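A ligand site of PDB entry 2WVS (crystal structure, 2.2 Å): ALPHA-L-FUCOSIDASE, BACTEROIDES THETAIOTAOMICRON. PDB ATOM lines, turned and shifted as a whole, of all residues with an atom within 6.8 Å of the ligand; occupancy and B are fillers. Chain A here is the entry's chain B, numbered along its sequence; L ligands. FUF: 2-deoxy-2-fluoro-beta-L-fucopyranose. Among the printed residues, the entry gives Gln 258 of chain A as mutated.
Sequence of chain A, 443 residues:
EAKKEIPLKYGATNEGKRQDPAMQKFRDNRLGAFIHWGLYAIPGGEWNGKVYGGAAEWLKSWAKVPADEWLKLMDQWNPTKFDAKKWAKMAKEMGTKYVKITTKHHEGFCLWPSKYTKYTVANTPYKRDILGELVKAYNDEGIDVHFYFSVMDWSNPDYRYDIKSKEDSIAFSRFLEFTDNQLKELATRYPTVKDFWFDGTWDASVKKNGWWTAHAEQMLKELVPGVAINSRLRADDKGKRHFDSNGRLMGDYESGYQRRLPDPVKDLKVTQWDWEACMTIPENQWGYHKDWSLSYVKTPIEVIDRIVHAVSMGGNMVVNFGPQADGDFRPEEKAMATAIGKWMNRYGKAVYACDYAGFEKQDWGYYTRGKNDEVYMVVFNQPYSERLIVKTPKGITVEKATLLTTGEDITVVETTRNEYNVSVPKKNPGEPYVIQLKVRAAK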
ATOM      1  N   PHE A  34     -24.801 -38.898 -24.496  1.00  0.00           N
ATOM      2  CA  PHE A  34     -24.607 -37.471 -24.207  1.00  0.00           C
ATOM      3  C   PHE A  34     -26.006 -36.813 -24.259  1.00  0.00           C
ATOM      4  O   PHE A  34     -26.811 -37.173 -25.123  1.00  0.00           O
ATOM      5  CB  PHE A  34     -23.719 -36.836 -25.262  1.00  0.00           C
ATOM      6  CG  PHE A  34     -22.739 -35.834 -24.710  1.00  0.00           C
ATOM      7  CD1 PHE A  34     -21.369 -35.958 -24.987  1.00  0.00           C
ATOM      8  CD2 PHE A  34     -23.163 -34.786 -23.911  1.00  0.00           C
ATOM      9  CE1 PHE A  34     -20.439 -35.033 -24.476  1.00  0.00           C
ATOM     10  CE2 PHE A  34     -22.241 -33.865 -23.390  1.00  0.00           C
ATOM     11  CZ  PHE A  34     -20.895 -33.993 -23.667  1.00  0.00           C
ATOM     12  N   HIS A  36     -27.491 -33.053 -24.804  1.00  0.00           N
ATOM     13  CA  HIS A  36     -27.439 -31.637 -25.090  1.00  0.00           C
ATOM     14  C   HIS A  36     -28.838 -31.052 -25.007  1.00  0.00           C
ATOM     15  O   HIS A  36     -29.697 -31.294 -25.870  1.00  0.00           O
ATOM     16  CB  HIS A  36     -26.863 -31.379 -26.471  1.00  0.00           C
ATOM     17  CG  HIS A  36     -25.382 -31.295 -26.480  1.00  0.00           C
ATOM     18  ND1 HIS A  36     -24.580 -32.410 -26.349  1.00  0.00           N
ATOM     19  CD2 HIS A  36     -24.548 -30.237 -26.597  1.00  0.00           C
ATOM     20  CE1 HIS A  36     -23.316 -32.042 -26.384  1.00  0.00           C
ATOM     21  NE2 HIS A  36     -23.265 -30.721 -26.536  1.00  0.00           N
ATOM     22  N   ALA A  55     -24.852 -26.068 -36.559  1.00  0.00           N
ATOM     23  CA  ALA A  55     -25.233 -26.751 -35.310  1.00  0.00           C
ATOM     24  C   ALA A  55     -26.259 -25.941 -34.508  1.00  0.00           C
ATOM     25  O   ALA A  55     -26.077 -24.744 -34.278  1.00  0.00           O
ATOM     26  CB  ALA A  55     -23.990 -27.010 -34.439  1.00  0.00           C
ATOM     27  N   GLU A  57     -27.252 -25.869 -31.311  1.00  0.00           N
ATOM     28  CA  GLU A  57     -26.806 -25.257 -30.056  1.00  0.00           C
ATOM     29  C   GLU A  57     -26.018 -23.949 -30.256  1.00  0.00           C
ATOM     30  O   GLU A  57     -25.886 -23.176 -29.323  1.00  0.00           O
ATOM     31  CB  GLU A  57     -26.029 -26.249 -29.165  1.00  0.00           C
ATOM     32  CG  GLU A  57     -24.598 -26.521 -29.635  1.00  0.00           C
ATOM     33  CD  GLU A  57     -24.507 -27.467 -30.840  1.00  0.00           C
ATOM     34  OE1 GLU A  57     -25.563 -27.933 -31.368  1.00  0.00           O
ATOM     35  OE2 GLU A  57     -23.349 -27.743 -31.231  1.00  0.00           O
ATOM     36  N   TRP A  58     -25.510 -23.729 -31.473  1.00  0.00           N
ATOM     37  CA  TRP A  58     -24.767 -22.497 -31.829  1.00  0.00           C
ATOM     38  C   TRP A  58     -25.627 -21.458 -32.575  1.00  0.00           C
ATOM     39  O   TRP A  58     -25.095 -20.487 -33.128  1.00  0.00           O
ATOM     40  CB  TRP A  58     -23.565 -22.850 -32.717  1.00  0.00           C
ATOM     41  CG  TRP A  58     -22.368 -23.321 -31.977  1.00  0.00           C
ATOM     42  CD1 TRP A  58     -22.181 -24.567 -31.385  1.00  0.00           C
ATOM     43  CD2 TRP A  58     -21.166 -22.576 -31.742  1.00  0.00           C
ATOM     44  NE1 TRP A  58     -20.948 -24.608 -30.779  1.00  0.00           N
ATOM     45  CE2 TRP A  58     -20.295 -23.423 -31.008  1.00  0.00           C
ATOM     46  CE3 TRP A  58     -20.739 -21.290 -32.109  1.00  0.00           C
ATOM     47  CZ2 TRP A  58     -19.013 -22.997 -30.602  1.00  0.00           C
ATOM     48  CZ3 TRP A  58     -19.460 -20.868 -31.716  1.00  0.00           C
ATOM     49  CH2 TRP A  58     -18.627 -21.718 -30.964  1.00  0.00           C
ATOM     50  N   THR A 102     -25.184 -31.690 -20.498  1.00  0.00           N
ATOM     51  CA  THR A 102     -24.841 -30.282 -20.553  1.00  0.00           C
ATOM     52  C   THR A 102     -25.478 -29.550 -19.350  1.00  0.00           C
ATOM     53  O   THR A 102     -26.679 -29.251 -19.357  1.00  0.00           O
ATOM     54  CB  THR A 102     -25.324 -29.632 -21.837  1.00  0.00           C
ATOM     55  OG1 THR A 102     -26.747 -29.827 -21.924  1.00  0.00           O
ATOM     56  CG2 THR A 102     -24.620 -30.246 -23.052  1.00  0.00           C
ATOM     57  N   HIS A 105     -24.397 -24.724 -21.444  1.00  0.00           N
ATOM     58  CA  HIS A 105     -23.715 -24.702 -22.739  1.00  0.00           C
ATOM     59  C   HIS A 105     -23.202 -23.254 -22.985  1.00  0.00           C
ATOM     60  O   HIS A 105     -23.277 -22.419 -22.062  1.00  0.00           O
ATOM     61  CB  HIS A 105     -24.632 -25.241 -23.849  1.00  0.00           C
ATOM     62  CG  HIS A 105     -23.874 -25.837 -25.000  1.00  0.00           C
ATOM     63  ND1 HIS A 105     -23.429 -25.097 -26.070  1.00  0.00           N
ATOM     64  CD2 HIS A 105     -23.440 -27.106 -25.215  1.00  0.00           C
ATOM     65  CE1 HIS A 105     -22.765 -25.880 -26.908  1.00  0.00           C
ATOM     66  NE2 HIS A 105     -22.766 -27.101 -26.412  1.00  0.00           N
ATOM     67  N   HIS A 106     -22.665 -22.947 -24.180  1.00  0.00           N
ATOM     68  CA  HIS A 106     -22.121 -21.599 -24.428  1.00  0.00           C
ATOM     69  C   HIS A 106     -23.074 -20.466 -24.072  1.00  0.00           C
ATOM     70  O   HIS A 106     -22.640 -19.414 -23.623  1.00  0.00           O
ATOM     71  CB  HIS A 106     -21.659 -21.409 -25.882  1.00  0.00           C
ATOM     72  CG  HIS A 106     -20.801 -22.522 -26.417  1.00  0.00           C
ATOM     73  ND1 HIS A 106     -19.840 -23.163 -25.652  1.00  0.00           N
ATOM     74  CD2 HIS A 106     -20.735 -23.080 -27.652  1.00  0.00           C
ATOM     75  CE1 HIS A 106     -19.223 -24.065 -26.398  1.00  0.00           C
ATOM     76  NE2 HIS A 106     -19.745 -24.025 -27.618  1.00  0.00           N
ATOM     77  N   TYR A 148     -21.053 -32.035 -18.447  1.00  0.00           N
ATOM     78  CA  TYR A 148     -20.510 -31.201 -19.508  1.00  0.00           C
ATOM     79  C   TYR A 148     -20.600 -29.809 -18.932  1.00  0.00           C
ATOM     80  O   TYR A 148     -21.568 -29.480 -18.264  1.00  0.00           O
ATOM     81  CB  TYR A 148     -21.370 -31.328 -20.782  1.00  0.00           C
ATOM     82  CG  TYR A 148     -21.138 -30.202 -21.750  1.00  0.00           C
ATOM     83  CD1 TYR A 148     -20.516 -30.440 -22.985  1.00  0.00           C
ATOM     84  CD2 TYR A 148     -21.523 -28.886 -21.425  1.00  0.00           C
ATOM     85  CE1 TYR A 148     -20.268 -29.375 -23.894  1.00  0.00           C
ATOM     86  CE2 TYR A 148     -21.249 -27.800 -22.316  1.00  0.00           C
ATOM     87  CZ  TYR A 148     -20.639 -28.069 -23.555  1.00  0.00           C
ATOM     88  OH  TYR A 148     -20.344 -27.016 -24.426  1.00  0.00           O
ATOM     89  N   MET A 152     -16.457 -20.865 -21.792  1.00  0.00           N
ATOM     90  CA  MET A 152     -17.078 -19.763 -22.580  1.00  0.00           C
ATOM     91  C   MET A 152     -18.546 -19.571 -22.207  1.00  0.00           C
ATOM     92  O   MET A 152     -19.297 -20.509 -22.146  1.00  0.00           O
ATOM     93  CB  MET A 152     -16.977 -20.049 -24.070  1.00  0.00           C
ATOM     94  CG  MET A 152     -17.776 -19.078 -24.949  1.00  0.00           C
ATOM     95  SD  MET A 152     -17.173 -19.154 -26.635  1.00  0.00           S
ATOM     96  CE  MET A 152     -17.856 -20.722 -27.129  1.00  0.00           C
ATOM     97  N   TRP A 197     -16.487 -32.557 -18.078  1.00  0.00           N
ATOM     98  CA  TRP A 197     -16.131 -32.495 -19.460  1.00  0.00           C
ATOM     99  C   TRP A 197     -16.242 -31.043 -19.911  1.00  0.00           C
ATOM    100  O   TRP A 197     -17.345 -30.553 -20.217  1.00  0.00           O
ATOM    101  CB  TRP A 197     -17.086 -33.348 -20.280  1.00  0.00           C
ATOM    102  CG  TRP A 197     -16.563 -33.805 -21.623  1.00  0.00           C
ATOM    103  CD1 TRP A 197     -15.857 -34.959 -21.888  1.00  0.00           C
ATOM    104  CD2 TRP A 197     -16.719 -33.143 -22.889  1.00  0.00           C
ATOM    105  NE1 TRP A 197     -15.570 -35.052 -23.238  1.00  0.00           N
ATOM    106  CE2 TRP A 197     -16.100 -33.968 -23.878  1.00  0.00           C
ATOM    107  CE3 TRP A 197     -17.345 -31.962 -23.289  1.00  0.00           C
ATOM    108  CZ2 TRP A 197     -16.083 -33.614 -25.250  1.00  0.00           C
ATOM    109  CZ3 TRP A 197     -17.322 -31.618 -24.652  1.00  0.00           C
ATOM    110  CH2 TRP A 197     -16.688 -32.436 -25.609  1.00  0.00           C
ATOM    111  N   PHE A 198     -15.099 -30.369 -19.950  1.00  0.00           N
ATOM    112  CA  PHE A 198     -15.096 -28.970 -20.324  1.00  0.00           C
ATOM    113  C   PHE A 198     -15.148 -28.752 -21.822  1.00  0.00           C
ATOM    114  O   PHE A 198     -14.647 -29.584 -22.604  1.00  0.00           O
ATOM    115  CB  PHE A 198     -13.891 -28.253 -19.741  1.00  0.00           C
ATOM    116  CG  PHE A 198     -13.939 -28.172 -18.244  1.00  0.00           C
ATOM    117  CD1 PHE A 198     -14.482 -27.049 -17.618  1.00  0.00           C
ATOM    118  CD2 PHE A 198     -13.488 -29.235 -17.469  1.00  0.00           C
ATOM    119  CE1 PHE A 198     -14.562 -26.988 -16.236  1.00  0.00           C
ATOM    120  CE2 PHE A 198     -13.565 -29.201 -16.095  1.00  0.00           C
ATOM    121  CZ  PHE A 198     -14.110 -28.065 -15.465  1.00  0.00           C
ATOM    122  N   ASP A 199     -15.741 -27.631 -22.206  1.00  0.00           N
ATOM    123  CA  ASP A 199     -15.807 -27.210 -23.591  1.00  0.00           C
ATOM    124  C   ASP A 199     -15.686 -25.658 -23.660  1.00  0.00           C
ATOM    125  O   ASP A 199     -15.772 -24.987 -22.650  1.00  0.00           O
ATOM    126  CB  ASP A 199     -17.159 -27.648 -24.180  1.00  0.00           C
ATOM    127  CG  ASP A 199     -17.157 -27.658 -25.708  1.00  0.00           C
ATOM    128  OD1 ASP A 199     -16.026 -27.572 -26.288  1.00  0.00           O
ATOM    129  OD2 ASP A 199     -18.247 -27.757 -26.326  1.00  0.00           O
ATOM    130  N   GLY A 200     -15.522 -25.112 -24.838  1.00  0.00           N
ATOM    131  CA  GLY A 200     -15.357 -23.662 -24.965  1.00  0.00           C
ATOM    132  C   GLY A 200     -14.174 -23.195 -24.144  1.00  0.00           C
ATOM    133  O   GLY A 200     -14.291 -22.281 -23.347  1.00  0.00           O
ATOM    134  N   TRP A 202     -11.034 -22.866 -25.914  1.00  0.00           N
ATOM    135  CA  TRP A 202     -10.046 -22.642 -26.997  1.00  0.00           C
ATOM    136  C   TRP A 202      -9.604 -21.194 -27.156  1.00  0.00           C
ATOM    137  O   TRP A 202      -8.659 -20.909 -27.905  1.00  0.00           O
ATOM    138  CB  TRP A 202     -10.590 -23.106 -28.361  1.00  0.00           C
ATOM    139  CG  TRP A 202     -12.002 -22.622 -28.624  1.00  0.00           C
ATOM    140  CD1 TRP A 202     -12.394 -21.371 -29.021  1.00  0.00           C
ATOM    141  CD2 TRP A 202     -13.204 -23.383 -28.453  1.00  0.00           C
ATOM    142  NE1 TRP A 202     -13.766 -21.307 -29.120  1.00  0.00           N
ATOM    143  CE2 TRP A 202     -14.285 -22.526 -28.773  1.00  0.00           C
ATOM    144  CE3 TRP A 202     -13.472 -24.712 -28.092  1.00  0.00           C
ATOM    145  CZ2 TRP A 202     -15.613 -22.963 -28.739  1.00  0.00           C
ATOM    146  CZ3 TRP A 202     -14.762 -25.133 -28.042  1.00  0.00           C
ATOM    147  CH2 TRP A 202     -15.836 -24.264 -28.352  1.00  0.00           C
ATOM    148  N   ARG A 232      -9.782 -31.532 -22.961  1.00  0.00           N
ATOM    149  CA  ARG A 232     -10.221 -30.304 -23.612  1.00  0.00           C
ATOM    150  C   ARG A 232     -10.132 -29.110 -22.661  1.00  0.00           C
ATOM    151  O   ARG A 232     -10.079 -27.975 -23.100  1.00  0.00           O
ATOM    152  CB  ARG A 232     -11.643 -30.476 -24.176  1.00  0.00           C
ATOM    153  CG  ARG A 232     -12.084 -29.425 -25.215  1.00  0.00           C
ATOM    154  CD  ARG A 232     -13.455 -29.722 -25.833  1.00  0.00           C
ATOM    155  NE  ARG A 232     -13.377 -30.358 -27.147  1.00  0.00           N
ATOM    156  CZ  ARG A 232     -14.279 -30.222 -28.138  1.00  0.00           C
ATOM    157  NH1 ARG A 232     -15.370 -29.463 -28.009  1.00  0.00           N
ATOM    158  NH2 ARG A 232     -14.088 -30.865 -29.282  1.00  0.00           N
ATOM    159  N   GLN A 258     -14.294 -36.562 -32.246  1.00  0.00           N
ATOM    160  CA  GLN A 258     -15.729 -36.419 -32.458  1.00  0.00           C
ATOM    161  C   GLN A 258     -15.825 -36.239 -33.948  1.00  0.00           C
ATOM    162  O   GLN A 258     -14.995 -35.535 -34.538  1.00  0.00           O
ATOM    163  CB  GLN A 258     -16.327 -35.252 -31.641  1.00  0.00           C
ATOM    164  CG  GLN A 258     -15.790 -33.828 -31.871  1.00  0.00           C
ATOM    165  CD  GLN A 258     -16.207 -32.837 -30.770  1.00  0.00           C
ATOM    166  OE1 GLN A 258     -16.190 -33.177 -29.570  1.00  0.00           O
ATOM    167  NE2 GLN A 258     -16.553 -31.624 -31.168  1.00  0.00           N
ATOM    168  N   CYS A 278     -16.941 -38.624 -28.556  1.00  0.00           N
ATOM    169  CA  CYS A 278     -18.351 -38.304 -28.538  1.00  0.00           C
ATOM    170  C   CYS A 278     -18.828 -38.034 -29.941  1.00  0.00           C
ATOM    171  O   CYS A 278     -18.145 -37.353 -30.691  1.00  0.00           O
ATOM    172  CB  CYS A 278     -18.607 -37.077 -27.682  1.00  0.00           C
ATOM    173  SG  CYS A 278     -17.804 -37.136 -26.059  1.00  0.00           S
ATOM    174  N   ASN A 284     -23.394 -32.971 -37.805  1.00  0.00           N
ATOM    175  CA  ASN A 284     -22.927 -31.973 -36.841  1.00  0.00           C
ATOM    176  C   ASN A 284     -24.058 -31.199 -36.138  1.00  0.00           C
ATOM    177  O   ASN A 284     -24.213 -29.984 -36.335  1.00  0.00           O
ATOM    178  CB  ASN A 284     -21.883 -31.030 -37.471  1.00  0.00           C
ATOM    179  CG  ASN A 284     -21.077 -30.255 -36.423  1.00  0.00           C
ATOM    180  OD1 ASN A 284     -20.751 -30.761 -35.337  1.00  0.00           O
ATOM    181  ND2 ASN A 284     -20.739 -29.016 -36.753  1.00  0.00           N
ATOM    182  N   TRP A 286     -25.685 -31.136 -32.140  1.00  0.00           N
ATOM    183  CA  TRP A 286     -25.670 -31.636 -30.742  1.00  0.00           C
ATOM    184  C   TRP A 286     -27.003 -31.356 -30.042  1.00  0.00           C
ATOM    185  O   TRP A 286     -27.687 -32.295 -29.566  1.00  0.00           O
ATOM    186  CB  TRP A 286     -24.449 -31.116 -29.954  1.00  0.00           C
ATOM    187  CG  TRP A 286     -23.080 -31.485 -30.592  1.00  0.00           C
ATOM    188  CD1 TRP A 286     -22.425 -30.807 -31.584  1.00  0.00           C
ATOM    189  CD2 TRP A 286     -22.212 -32.589 -30.252  1.00  0.00           C
ATOM    190  NE1 TRP A 286     -21.246 -31.419 -31.899  1.00  0.00           N
ATOM    191  CE2 TRP A 286     -21.076 -32.511 -31.089  1.00  0.00           C
ATOM    192  CE3 TRP A 286     -22.305 -33.648 -29.340  1.00  0.00           C
ATOM    193  CZ2 TRP A 286     -20.036 -33.432 -31.036  1.00  0.00           C
ATOM    194  CZ3 TRP A 286     -21.251 -34.578 -29.273  1.00  0.00           C
ATOM    195  CH2 TRP A 286     -20.144 -34.467 -30.134  1.00  0.00           C
ATOM    196  N   GLY A 287     -27.354 -30.070 -29.982  1.00  0.00           N
ATOM    197  CA  GLY A 287     -28.675 -29.642 -29.533  1.00  0.00           C
ATOM    198  C   GLY A 287     -29.722 -30.025 -30.579  1.00  0.00           C
ATOM    199  O   GLY A 287     -29.382 -30.379 -31.716  1.00  0.00           O
ATOM    200  N   ASN A 320     -24.538 -38.975 -28.702  1.00  0.00           N
ATOM    201  CA  ASN A 320     -25.332 -37.788 -28.394  1.00  0.00           C
ATOM    202  C   ASN A 320     -26.824 -37.844 -28.739  1.00  0.00           C
ATOM    203  O   ASN A 320     -27.217 -38.455 -29.735  1.00  0.00           O
ATOM    204  CB  ASN A 320     -24.711 -36.566 -29.034  1.00  0.00           C
ATOM    205  CG  ASN A 320     -25.443 -35.299 -28.667  1.00  0.00           C
ATOM    206  OD1 ASN A 320     -25.300 -34.803 -27.566  1.00  0.00           O
ATOM    207  ND2 ASN A 320     -26.265 -34.779 -29.577  1.00  0.00           N
HETATM  208  C1  FUF L   1     -18.370 -28.249 -27.668  1.00  0.00           C
HETATM  209  C2  FUF L   1     -19.261 -27.380 -28.600  1.00  0.00           C
HETATM  210  C3  FUF L   1     -20.306 -28.187 -29.373  1.00  0.00           C
HETATM  211  C4  FUF L   1     -20.749 -29.435 -28.589  1.00  0.00           C
HETATM  212  C5  FUF L   1     -19.521 -30.379 -28.494  1.00  0.00           C
HETATM  213  C6  FUF L   1     -19.659 -31.564 -27.511  1.00  0.00           C
HETATM  214  F2  FUF L   1     -18.572 -26.500 -29.409  1.00  0.00           F
HETATM  215  O3  FUF L   1     -21.373 -27.296 -29.531  1.00  0.00           O
HETATM  216  O4  FUF L   1     -21.245 -29.082 -27.260  1.00  0.00           O
HETATM  217  O5  FUF L   1     -18.288 -29.585 -28.281  1.00  0.00           O
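NE2 of His 106 sits close to F2 of the ligand, 3.3 Å away.
CE1 of Tyr 148 touches O4 of the ligand, 3.5 Å away.
Trp 197 touches the ligand (CH2 to C6, 3.6 Å).
Trp 202 touches the ligand.
Gln 258 touches the ligand.
Trp 286 touches the ligand.
Of the 22 residues printed, 12 come within 4 Å of the ligand.
The nearest printed residue that does not touch the ligand is Phe 34 (4.7 Å).
The side-chain carboxylate (OD2) of Asp 199 is bonded to a carbon (C1) of the ligand (1.4 Å).
A ring nitrogen (NE2) of His 105 sits at hydrogen-bond distance from an oxygen (O4) of the ligand (2.6 Å).
The side-chain carboxylate (OE2) of Glu 57 lies within hydrogen-bond range of an oxygen (O3) of the ligand.
O4 of the ligand sits at hydrogen-bond distance from NE2 of His 36 (2.7 Å).
The guanidinium group of Arg 232 sits at hydrogen-bond distance from an oxygen (O5) of the ligand (2.9 Å).
O3 of the ligand sits at hydrogen-bond distance from NE1 of Trp 58 (3.0 Å).
OD1 of Asp 199 is in salt-bridge range of NH1 of Arg 232.
The side-chain hydroxyl (OH) of Tyr 148 is in hydrogen-bond range of a ring nitrogen (NE2) of His 105 (3.1 Å).
The backbone NH (N) of Trp 286 sits at hydrogen-bond distance from the side-chain carboxylate (OE1) of Glu 57, 3.3 Å away.
The backbone NH (N) of Gly 287 lies within hydrogen-bond range of the side-chain carboxylate (OE1) of Glu 57.
OD1 of Asn 320 is in hydrogen-bond range of ND1 of His 36.
NH2 of Arg 232 is in hydrogen-bond range of OE1 of Gln 258 (3.1 Å).
NE1 of Trp 58 sits close to NE2 of His 106 (3.4 Å).
O of Trp 286 sits at hydrogen-bond distance from ND2 of Asn 320 (2.9 Å).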
